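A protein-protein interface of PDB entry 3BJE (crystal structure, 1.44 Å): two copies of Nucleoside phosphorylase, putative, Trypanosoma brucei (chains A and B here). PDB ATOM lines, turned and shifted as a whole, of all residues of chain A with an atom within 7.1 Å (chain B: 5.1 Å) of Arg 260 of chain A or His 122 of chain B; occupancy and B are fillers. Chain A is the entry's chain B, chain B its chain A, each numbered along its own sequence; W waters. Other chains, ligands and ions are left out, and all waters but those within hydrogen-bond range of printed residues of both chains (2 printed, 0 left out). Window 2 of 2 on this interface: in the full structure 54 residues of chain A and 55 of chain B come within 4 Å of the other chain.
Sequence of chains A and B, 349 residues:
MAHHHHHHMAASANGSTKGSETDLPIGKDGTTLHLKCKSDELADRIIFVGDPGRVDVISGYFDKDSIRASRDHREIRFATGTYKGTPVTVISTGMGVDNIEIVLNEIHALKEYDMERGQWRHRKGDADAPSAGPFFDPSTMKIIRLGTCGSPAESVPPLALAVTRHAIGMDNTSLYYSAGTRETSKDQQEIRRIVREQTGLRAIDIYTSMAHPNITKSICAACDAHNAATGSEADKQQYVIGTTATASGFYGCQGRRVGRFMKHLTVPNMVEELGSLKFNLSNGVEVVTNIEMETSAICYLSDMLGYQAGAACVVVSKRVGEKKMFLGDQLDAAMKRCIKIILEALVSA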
ATOM      1  N   ARG A 257     -13.607 -21.594 -11.429  1.00  0.00           N
ATOM      2  CA  ARG A 257     -14.719 -21.030 -10.688  1.00  0.00           C
ATOM      3  C   ARG A 257     -15.559 -22.124 -10.044  1.00  0.00           C
ATOM      4  O   ARG A 257     -16.204 -22.904 -10.735  1.00  0.00           O
ATOM      5  CB  ARG A 257     -15.600 -20.230 -11.642  1.00  0.00           C
ATOM      6  CG  ARG A 257     -14.915 -18.993 -12.240  1.00  0.00           C
ATOM      7  CD  ARG A 257     -14.149 -19.346 -13.517  1.00  0.00           C
ATOM      8  NE  ARG A 257     -13.712 -18.158 -14.257  1.00  0.00           N
ATOM      9  CZ  ARG A 257     -14.502 -17.416 -15.035  1.00  0.00           C
ATOM     10  NH1 ARG A 257     -15.787 -17.726 -15.199  1.00  0.00           N
ATOM     11  NH2 ARG A 257     -14.005 -16.352 -15.659  1.00  0.00           N
ATOM     12  N   VAL A 258     -15.513 -22.196  -8.717  1.00  0.00           N
ATOM     13  CA  VAL A 258     -16.145 -23.294  -7.971  1.00  0.00           C
ATOM     14  C   VAL A 258     -17.071 -22.777  -6.866  1.00  0.00           C
ATOM     15  O   VAL A 258     -16.616 -22.188  -5.904  1.00  0.00           O
ATOM     16  CB  VAL A 258     -15.100 -24.250  -7.348  1.00  0.00           C
ATOM     17  CG1 VAL A 258     -15.787 -25.428  -6.664  1.00  0.00           C
ATOM     18  CG2 VAL A 258     -14.111 -24.742  -8.426  1.00  0.00           C
ATOM     19  N   GLY A 259     -18.375 -22.978  -7.044  1.00  0.00           N
ATOM     20  CA  GLY A 259     -19.345 -22.699  -6.000  1.00  0.00           C
ATOM     21  C   GLY A 259     -19.176 -21.370  -5.308  1.00  0.00           C
ATOM     22  O   GLY A 259     -19.088 -20.316  -5.945  1.00  0.00           O
ATOM     23  N   ARG A 260     -19.112 -21.431  -3.987  1.00  0.00           N
ATOM     24  CA  ARG A 260     -19.123 -20.239  -3.160  1.00  0.00           C
ATOM     25  C   ARG A 260     -17.773 -19.541  -3.129  1.00  0.00           C
ATOM     26  O   ARG A 260     -17.650 -18.468  -2.532  1.00  0.00           O
ATOM     27  CB  ARG A 260     -19.551 -20.595  -1.736  1.00  0.00           C
ATOM     28  CG  ARG A 260     -20.937 -21.210  -1.625  1.00  0.00           C
ATOM     29  CD  ARG A 260     -22.042 -20.191  -1.860  1.00  0.00           C
ATOM     30  NE  ARG A 260     -23.335 -20.847  -1.990  1.00  0.00           N
ATOM     31  CZ  ARG A 260     -24.507 -20.226  -1.887  1.00  0.00           C
ATOM     32  NH1 ARG A 260     -24.560 -18.921  -1.666  1.00  0.00           N
ATOM     33  NH2 ARG A 260     -25.631 -20.916  -2.009  1.00  0.00           N
ATOM     34  N   PHE A 261     -16.760 -20.132  -3.759  1.00  0.00           N
ATOM     35  CA  PHE A 261     -15.455 -19.478  -3.878  1.00  0.00           C
ATOM     36  C   PHE A 261     -15.388 -18.470  -5.023  1.00  0.00           C
ATOM     37  O   PHE A 261     -14.589 -17.529  -5.004  1.00  0.00           O
ATOM     38  CB  PHE A 261     -14.348 -20.507  -4.138  1.00  0.00           C
ATOM     39  CG  PHE A 261     -13.909 -21.282  -2.933  1.00  0.00           C
ATOM     40  CD1 PHE A 261     -13.525 -20.640  -1.768  1.00  0.00           C
ATOM     41  CD2 PHE A 261     -13.793 -22.664  -2.995  1.00  0.00           C
ATOM     42  CE1 PHE A 261     -13.079 -21.364  -0.688  1.00  0.00           C
ATOM     43  CE2 PHE A 261     -13.341 -23.384  -1.923  1.00  0.00           C
ATOM     44  CZ  PHE A 261     -12.989 -22.727  -0.756  1.00  0.00           C
ATOM     45  N   MET A 262     -16.214 -18.677  -6.033  1.00  0.00           N
ATOM     46  CA  MET A 262     -16.051 -17.937  -7.274  1.00  0.00           C
ATOM     47  C   MET A 262     -16.014 -16.426  -7.051  1.00  0.00           C
ATOM     48  O   MET A 262     -15.191 -15.748  -7.662  1.00  0.00           O
ATOM     49  CB  MET A 262     -17.134 -18.316  -8.288  1.00  0.00           C
ATOM     50  CG  MET A 262     -17.091 -17.502  -9.569  1.00  0.00           C
ATOM     51  SD  MET A 262     -17.967 -15.930  -9.434  1.00  0.00           S
ATOM     52  CE  MET A 262     -19.673 -16.478  -9.522  1.00  0.00           C
ATOM     53  N   LYS A 263     -16.872 -15.909  -6.180  1.00  0.00           N
ATOM     54  CA  LYS A 263     -16.971 -14.452  -5.991  1.00  0.00           C
ATOM     55  C   LYS A 263     -15.761 -13.848  -5.280  1.00  0.00           C
ATOM     56  O   LYS A 263     -15.592 -12.634  -5.249  1.00  0.00           O
ATOM     57  CB  LYS A 263     -18.258 -14.078  -5.238  1.00  0.00           C
ATOM     58  CG  LYS A 263     -18.330 -14.572  -3.802  1.00  0.00           C
ATOM     59  CD  LYS A 263     -19.670 -14.208  -3.131  1.00  0.00           C
ATOM     60  CE  LYS A 263     -19.600 -12.905  -2.343  1.00  0.00           C
ATOM     61  NZ  LYS A 263     -20.858 -12.654  -1.539  1.00  0.00           N
ATOM     62  N   HIS A 264     -14.923 -14.707  -4.714  1.00  0.00           N
ATOM     63  CA  HIS A 264     -13.777 -14.271  -3.926  1.00  0.00           C
ATOM     64  C   HIS A 264     -12.453 -14.435  -4.678  1.00  0.00           C
ATOM     65  O   HIS A 264     -11.390 -14.165  -4.103  1.00  0.00           O
ATOM     66  CB  HIS A 264     -13.712 -15.082  -2.640  1.00  0.00           C
ATOM     67  CG  HIS A 264     -14.921 -14.938  -1.781  1.00  0.00           C
ATOM     68  ND1 HIS A 264     -15.252 -13.751  -1.165  1.00  0.00           N
ATOM     69  CD2 HIS A 264     -15.870 -15.834  -1.421  1.00  0.00           C
ATOM     70  CE1 HIS A 264     -16.365 -13.921  -0.470  1.00  0.00           C
ATOM     71  NE2 HIS A 264     -16.758 -15.176  -0.607  1.00  0.00           N
ATOM     72  N   HIS B 108     -16.129 -29.062  -0.870  1.00  0.00           N
ATOM     73  CA  HIS B 108     -17.186 -28.070  -1.149  1.00  0.00           C
ATOM     74  C   HIS B 108     -18.163 -28.541  -2.204  1.00  0.00           C
ATOM     75  O   HIS B 108     -19.376 -28.491  -1.972  1.00  0.00           O
ATOM     76  CB  HIS B 108     -16.563 -26.720  -1.518  1.00  0.00           C
ATOM     77  CG  HIS B 108     -17.558 -25.635  -1.753  1.00  0.00           C
ATOM     78  ND1 HIS B 108     -18.600 -25.396  -0.887  1.00  0.00           N
ATOM     79  CD2 HIS B 108     -17.677 -24.727  -2.755  1.00  0.00           C
ATOM     80  CE1 HIS B 108     -19.326 -24.388  -1.352  1.00  0.00           C
ATOM     81  NE2 HIS B 108     -18.791 -23.970  -2.485  1.00  0.00           N
ATOM     82  N   GLU B 112     -22.021 -29.410  -1.470  1.00  0.00           N
ATOM     83  CA  GLU B 112     -22.945 -28.343  -1.881  1.00  0.00           C
ATOM     84  C   GLU B 112     -23.321 -28.322  -3.366  1.00  0.00           C
ATOM     85  O   GLU B 112     -24.207 -27.552  -3.764  1.00  0.00           O
ATOM     86  CB  GLU B 112     -22.412 -26.989  -1.435  1.00  0.00           C
ATOM     87  CG  GLU B 112     -22.321 -26.849   0.066  1.00  0.00           C
ATOM     88  CD  GLU B 112     -22.028 -25.433   0.508  1.00  0.00           C
ATOM     89  OE1 GLU B 112     -22.797 -24.512   0.120  1.00  0.00           O
ATOM     90  OE2 GLU B 112     -21.061 -25.244   1.279  1.00  0.00           O
ATOM     91  N   TRP B 120     -26.062 -25.932  -7.451  1.00  0.00           N
ATOM     92  CA  TRP B 120     -25.542 -25.697  -6.113  1.00  0.00           C
ATOM     93  C   TRP B 120     -26.686 -25.504  -5.124  1.00  0.00           C
ATOM     94  O   TRP B 120     -27.703 -24.890  -5.430  1.00  0.00           O
ATOM     95  CB  TRP B 120     -24.587 -24.491  -6.101  1.00  0.00           C
ATOM     96  CG  TRP B 120     -23.325 -24.767  -6.852  1.00  0.00           C
ATOM     97  CD1 TRP B 120     -23.110 -24.593  -8.191  1.00  0.00           C
ATOM     98  CD2 TRP B 120     -22.106 -25.304  -6.321  1.00  0.00           C
ATOM     99  NE1 TRP B 120     -21.834 -24.976  -8.524  1.00  0.00           N
ATOM    100  CE2 TRP B 120     -21.198 -25.418  -7.397  1.00  0.00           C
ATOM    101  CE3 TRP B 120     -21.686 -25.691  -5.041  1.00  0.00           C
ATOM    102  CZ2 TRP B 120     -19.912 -25.912  -7.239  1.00  0.00           C
ATOM    103  CZ3 TRP B 120     -20.390 -26.184  -4.882  1.00  0.00           C
ATOM    104  CH2 TRP B 120     -19.523 -26.292  -5.977  1.00  0.00           C
ATOM    105  N   ARG B 121     -26.510 -26.049  -3.932  1.00  0.00           N
ATOM    106  CA  ARG B 121     -27.519 -25.970  -2.897  1.00  0.00           C
ATOM    107  C   ARG B 121     -27.690 -24.538  -2.424  1.00  0.00           C
ATOM    108  O   ARG B 121     -26.735 -23.765  -2.416  1.00  0.00           O
ATOM    109  CB  ARG B 121     -27.105 -26.854  -1.720  1.00  0.00           C
ATOM    110  CG  ARG B 121     -27.030 -28.346  -2.060  1.00  0.00           C
ATOM    111  CD  ARG B 121     -26.650 -29.195  -0.851  1.00  0.00           C
ATOM    112  NE  ARG B 121     -26.354 -30.557  -1.274  1.00  0.00           N
ATOM    113  CZ  ARG B 121     -27.266 -31.464  -1.617  1.00  0.00           C
ATOM    114  NH1 ARG B 121     -28.565 -31.187  -1.563  1.00  0.00           N
ATOM    115  NH2 ARG B 121     -26.877 -32.669  -2.015  1.00  0.00           N
ATOM    116  N   HIS B 122     -28.909 -24.185  -2.022  1.00  0.00           N
ATOM    117  CA  HIS B 122     -29.179 -22.852  -1.510  1.00  0.00           C
ATOM    118  C   HIS B 122     -28.612 -22.729  -0.116  1.00  0.00           C
ATOM    119  O   HIS B 122     -28.522 -23.715   0.621  1.00  0.00           O
ATOM    120  CB  HIS B 122     -30.679 -22.558  -1.401  1.00  0.00           C
ATOM    121  CG  HIS B 122     -31.437 -22.752  -2.670  1.00  0.00           C
ATOM    122  ND1 HIS B 122     -31.146 -22.058  -3.821  1.00  0.00           N
ATOM    123  CD2 HIS B 122     -32.483 -23.559  -2.966  1.00  0.00           C
ATOM    124  CE1 HIS B 122     -31.980 -22.432  -4.777  1.00  0.00           C
ATOM    125  NE2 HIS B 122     -32.806 -23.338  -4.283  1.00  0.00           N
ATOM    126  N   ARG B 123     -28.268 -21.497   0.238  1.00  0.00           N
ATOM    127  CA  ARG B 123     -27.946 -21.135   1.608  1.00  0.00           C
ATOM    128  C   ARG B 123     -28.876 -20.013   2.038  1.00  0.00           C
ATOM    129  O   ARG B 123     -29.374 -19.253   1.205  1.00  0.00           O
ATOM    130  CB  ARG B 123     -26.517 -20.651   1.702  1.00  0.00           C
ATOM    131  CG  ARG B 123     -25.478 -21.713   1.494  1.00  0.00           C
ATOM    132  CD  ARG B 123     -24.150 -21.088   1.711  1.00  0.00           C
ATOM    133  NE  ARG B 123     -23.027 -22.013   1.626  1.00  0.00           N
ATOM    134  CZ  ARG B 123     -21.803 -21.680   2.023  1.00  0.00           C
ATOM    135  NH1 ARG B 123     -21.577 -20.493   2.580  1.00  0.00           N
ATOM    136  NH2 ARG B 123     -20.816 -22.549   1.923  1.00  0.00           N
ATOM    137  N   LYS B 124     -29.102 -19.907   3.342  1.00  0.00           N
ATOM    138  CA  LYS B 124     -29.961 -18.853   3.876  1.00  0.00           C
ATOM    139  C   LYS B 124     -29.411 -17.487   3.475  1.00  0.00           C
ATOM    140  O   LYS B 124     -28.210 -17.242   3.560  1.00  0.00           O
ATOM    141  CB  LYS B 124     -30.087 -18.972   5.396  1.00  0.00           C
ATOM    142  CG  LYS B 124     -30.924 -20.172   5.824  1.00  0.00           C
ATOM    143  CD  LYS B 124     -31.434 -20.048   7.253  1.00  0.00           C
ATOM    144  CE  LYS B 124     -32.357 -21.212   7.609  1.00  0.00           C
ATOM    145  NZ  LYS B 124     -32.976 -21.067   8.959  1.00  0.00           N
ATOM    146  N   ASP B 126     -29.559 -16.295   0.322  1.00  0.00           N
ATOM    147  CA  ASP B 126     -29.488 -16.243  -1.140  1.00  0.00           C
ATOM    148  C   ASP B 126     -30.674 -15.468  -1.696  1.00  0.00           C
ATOM    149  O   ASP B 126     -31.814 -15.732  -1.324  1.00  0.00           O
ATOM    150  CB  ASP B 126     -29.481 -17.644  -1.750  1.00  0.00           C
ATOM    151  CG  ASP B 126     -28.169 -18.367  -1.538  1.00  0.00           C
ATOM    152  OD1 ASP B 126     -27.205 -17.744  -1.049  1.00  0.00           O
ATOM    153  OD2 ASP B 126     -28.111 -19.564  -1.855  1.00  0.00           O
ATOM    154  N   ASP B 128     -32.254 -15.245  -4.797  1.00  0.00           N
ATOM    155  CA  ASP B 128     -33.309 -15.886  -5.583  1.00  0.00           C
ATOM    156  C   ASP B 128     -33.627 -17.320  -5.153  1.00  0.00           C
ATOM    157  O   ASP B 128     -34.176 -18.098  -5.936  1.00  0.00           O
ATOM    158  CB  ASP B 128     -32.944 -15.835  -7.070  1.00  0.00           C
ATOM    159  CG  ASP B 128     -32.639 -14.423  -7.546  1.00  0.00           C
ATOM    160  OD1 ASP B 128     -33.422 -13.502  -7.221  1.00  0.00           O
ATOM    161  OD2 ASP B 128     -31.611 -14.236  -8.235  1.00  0.00           O
ATOM    162  N   ALA B 129     -33.305 -17.666  -3.908  1.00  0.00           N
ATOM    163  CA  ALA B 129     -33.666 -18.970  -3.365  1.00  0.00           C
ATOM    164  C   ALA B 129     -35.122 -18.947  -2.910  1.00  0.00           C
ATOM    165  O   ALA B 129     -35.600 -17.925  -2.412  1.00  0.00           O
ATOM    166  CB  ALA B 129     -32.765 -19.332  -2.203  1.00  0.00           C
ATOM    167  N   PRO B 130     -35.837 -20.074  -3.075  1.00  0.00           N
ATOM    168  CA  PRO B 130     -37.153 -20.196  -2.460  1.00  0.00           C
ATOM    169  C   PRO B 130     -37.079 -19.993  -0.950  1.00  0.00           C
ATOM    170  O   PRO B 130     -36.112 -20.415  -0.319  1.00  0.00           O
ATOM    171  CB  PRO B 130     -37.563 -21.638  -2.779  1.00  0.00           C
ATOM    172  CG  PRO B 130     -36.748 -22.030  -3.947  1.00  0.00           C
ATOM    173  CD  PRO B 130     -35.464 -21.282  -3.834  1.00  0.00           C
ATOM    174  N   GLY B 133     -36.431 -23.116   0.844  1.00  0.00           N
ATOM    175  CA  GLY B 133     -35.128 -23.740   0.593  1.00  0.00           C
ATOM    176  C   GLY B 133     -35.292 -24.957  -0.306  1.00  0.00           C
ATOM    177  O   GLY B 133     -35.917 -24.857  -1.362  1.00  0.00           O
ATOM    178  N   PRO B 134     -34.749 -26.122   0.100  1.00  0.00           N
ATOM    179  CA  PRO B 134     -34.023 -26.395   1.344  1.00  0.00           C
ATOM    180  C   PRO B 134     -32.720 -25.604   1.398  1.00  0.00           C
ATOM    181  O   PRO B 134     -32.247 -25.129   0.359  1.00  0.00           O
ATOM    182  CB  PRO B 134     -33.712 -27.898   1.267  1.00  0.00           C
ATOM    183  CG  PRO B 134     -34.520 -28.439   0.155  1.00  0.00           C
ATOM    184  CD  PRO B 134     -34.815 -27.308  -0.771  1.00  0.00           C
ATOM    185  N   PHE B 135     -32.159 -25.456   2.596  1.00  0.00           N
ATOM    186  CA  PHE B 135     -30.902 -24.735   2.763  1.00  0.00           C
ATOM    187  C   PHE B 135     -29.809 -25.622   3.322  1.00  0.00           C
ATOM    188  O   PHE B 135     -30.042 -26.440   4.216  1.00  0.00           O
ATOM    189  CB  PHE B 135     -31.087 -23.537   3.683  1.00  0.00           C
ATOM    190  CG  PHE B 135     -32.110 -22.565   3.192  1.00  0.00           C
ATOM    191  CD1 PHE B 135     -31.869 -21.804   2.058  1.00  0.00           C
ATOM    192  CD2 PHE B 135     -33.321 -22.419   3.856  1.00  0.00           C
ATOM    193  CE1 PHE B 135     -32.812 -20.910   1.591  1.00  0.00           C
ATOM    194  CE2 PHE B 135     -34.268 -21.522   3.403  1.00  0.00           C
ATOM    195  CZ  PHE B 135     -34.015 -20.766   2.268  1.00  0.00           C
ATOM    196  N   PHE B 136     -28.611 -25.453   2.778  1.00  0.00           N
ATOM    197  CA  PHE B 136     -27.438 -26.077   3.345  1.00  0.00           C
ATOM    198  C   PHE B 136     -26.854 -25.170   4.426  1.00  0.00           C
ATOM    199  O   PHE B 136     -26.653 -23.981   4.187  1.00  0.00           O
ATOM    200  CB  PHE B 136     -26.397 -26.320   2.259  1.00  0.00           C
ATOM    201  CG  PHE B 136     -25.173 -27.000   2.757  1.00  0.00           C
ATOM    202  CD1 PHE B 136     -25.150 -28.378   2.908  1.00  0.00           C
ATOM    203  CD2 PHE B 136     -24.031 -26.261   3.073  1.00  0.00           C
ATOM    204  CE1 PHE B 136     -24.018 -29.017   3.374  1.00  0.00           C
ATOM    205  CE2 PHE B 136     -22.900 -26.892   3.549  1.00  0.00           C
ATOM    206  CZ  PHE B 136     -22.886 -28.270   3.696  1.00  0.00           C
ATOM    207  N   LEU B 305     -15.762 -20.428   3.353  1.00  0.00           N
ATOM    208  CA  LEU B 305     -16.955 -21.241   3.049  1.00  0.00           C
ATOM    209  C   LEU B 305     -17.973 -21.304   4.189  1.00  0.00           C
ATOM    210  O   LEU B 305     -19.079 -21.806   3.994  1.00  0.00           O
ATOM    211  CB  LEU B 305     -16.568 -22.671   2.689  1.00  0.00           C
ATOM    212  CG  LEU B 305     -15.753 -22.844   1.427  1.00  0.00           C
ATOM    213  CD1 LEU B 305     -15.388 -24.315   1.279  1.00  0.00           C
ATOM    214  CD2 LEU B 305     -16.539 -22.322   0.238  1.00  0.00           C
HETATM  215  O   HOH W   1     -19.076 -23.675  -9.859  1.00  0.00           O
HETATM  216  O   HOH W   2     -24.020 -23.728  -2.262  1.00  0.00           O
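O of Arg 121 of chain B sits at hydrogen-bond distance from NH2 of Arg 260 of chain A (3.1 Å). A ring nitrogen (NE2) of His 108 of chain B sits at hydrogen-bond distance from the backbone NH (N) of Arg 260 of chain A. The side-chain carboxylate (OD2) of Asp 126 of chain B lies within salt-bridge range of the guanidinium group (NH2) of Arg 260 of chain A, 2.8 Å away.
The guanidinium group (NH2) of Arg 123 of chain B lies within salt-bridge range of the side-chain carboxylate (OE2) of Glu 112 of chain B (2.8 Å). The guanidinium group (NH2) of Arg 123 of chain B lies within hydrogen-bond range of the backbone carbonyl oxygen (O) of Leu 305 of chain B, 2.8 Å away. The side-chain carboxylate (OE2) of Glu 112 of chain B lies close to a ring nitrogen (ND1) of His 108 of chain B (3.3 Å). The backbone NH of Arg 123 of chain B is in hydrogen-bond range of the side-chain carboxylate of Asp 126 of chain B (2.9 Å). O of Glu 112 of chain B lies within hydrogen-bond range of N of Arg 121 of chain B (2.8 Å). The backbone carbonyl oxygen (O) of His 122 of chain B lies within hydrogen-bond range of the backbone NH (N) of Phe 136 of chain B (2.8 Å).
Among the printed residues, pairs that only touch across the chains: Gly 259 of chain A with Trp 120 of chain B (3.3 Å), Arg 260 of chain A with Arg 123 of chain B (3.5 Å), Phe 261 of chain A with Leu 305 of chain B (3.5 Å), Gly 259 of chain A with His 108 of chain B (3.8 Å), Val 258 of chain A with Trp 120 of chain B (3.9 Å), Arg 260 of chain A with His 122 of chain B (3.97 Å) and Arg 260 of chain A with Leu 305 of chain B (3.99 Å).
His 122 of chain B touches one residue of chain A. Of the printed residues of chain A, Asp 126 of chain B touches Arg 260. Of the printed residues of chain A, Arg 121 of chain B touches Arg 260 (3.1 Å). Of the printed residues of chain A, Trp 120 of chain B touches Val 258 (3.9 Å) and Gly 259 (3.3 Å). Met 262 of chain A touches none of the printed residues of chain B. His 264 of chain A touches none of the printed residues of chain B. The nearest printed residue of chain B that does not touch Arg 260 of chain A is Glu 112 of chain B (4.2 Å). The nearest printed residue of chain A that does not touch His 122 of chain B is Gly 259 of chain A (10.5 Å). The nearest printed residue of chain B that does not touch Phe 261 of chain A is His 108 of chain B (4.4 Å).
Printed residues of chain B that touch a printed residue of chain A: His 108, Trp 120, Arg 121, His 122, Arg 123, Asp 126 and Leu 305. Among the printed residues, 10 pairs touch across the chains. Among the printed residues, Asp or Glu carboxylates within 4 Å of a Lys or Arg side-chain nitrogen of the other chain: Arg 260 of chain A with Asp 126 of chain B (2.8 Å).
No position is printed for both chains. Of the 10 pairs that touch across the chains among the printed residues, none has its exchanged pair printed and touching as well.
Water W2 lies within hydrogen-bond range of O of Arg 121 of chain B (2.7 Å), OE1 of Glu 112 of chain B (2.8 Å) and NE of Arg 260 of chain A (3.0 Å). Water W1 lies within hydrogen-bond range of the backbone NH of Gly 259 of chain A (3.0 Å), the backbone carbonyl oxygen of Arg 257 of chain A (3.1 Å) and the indole nitrogen of Trp 120 of chain B (3.3 Å).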
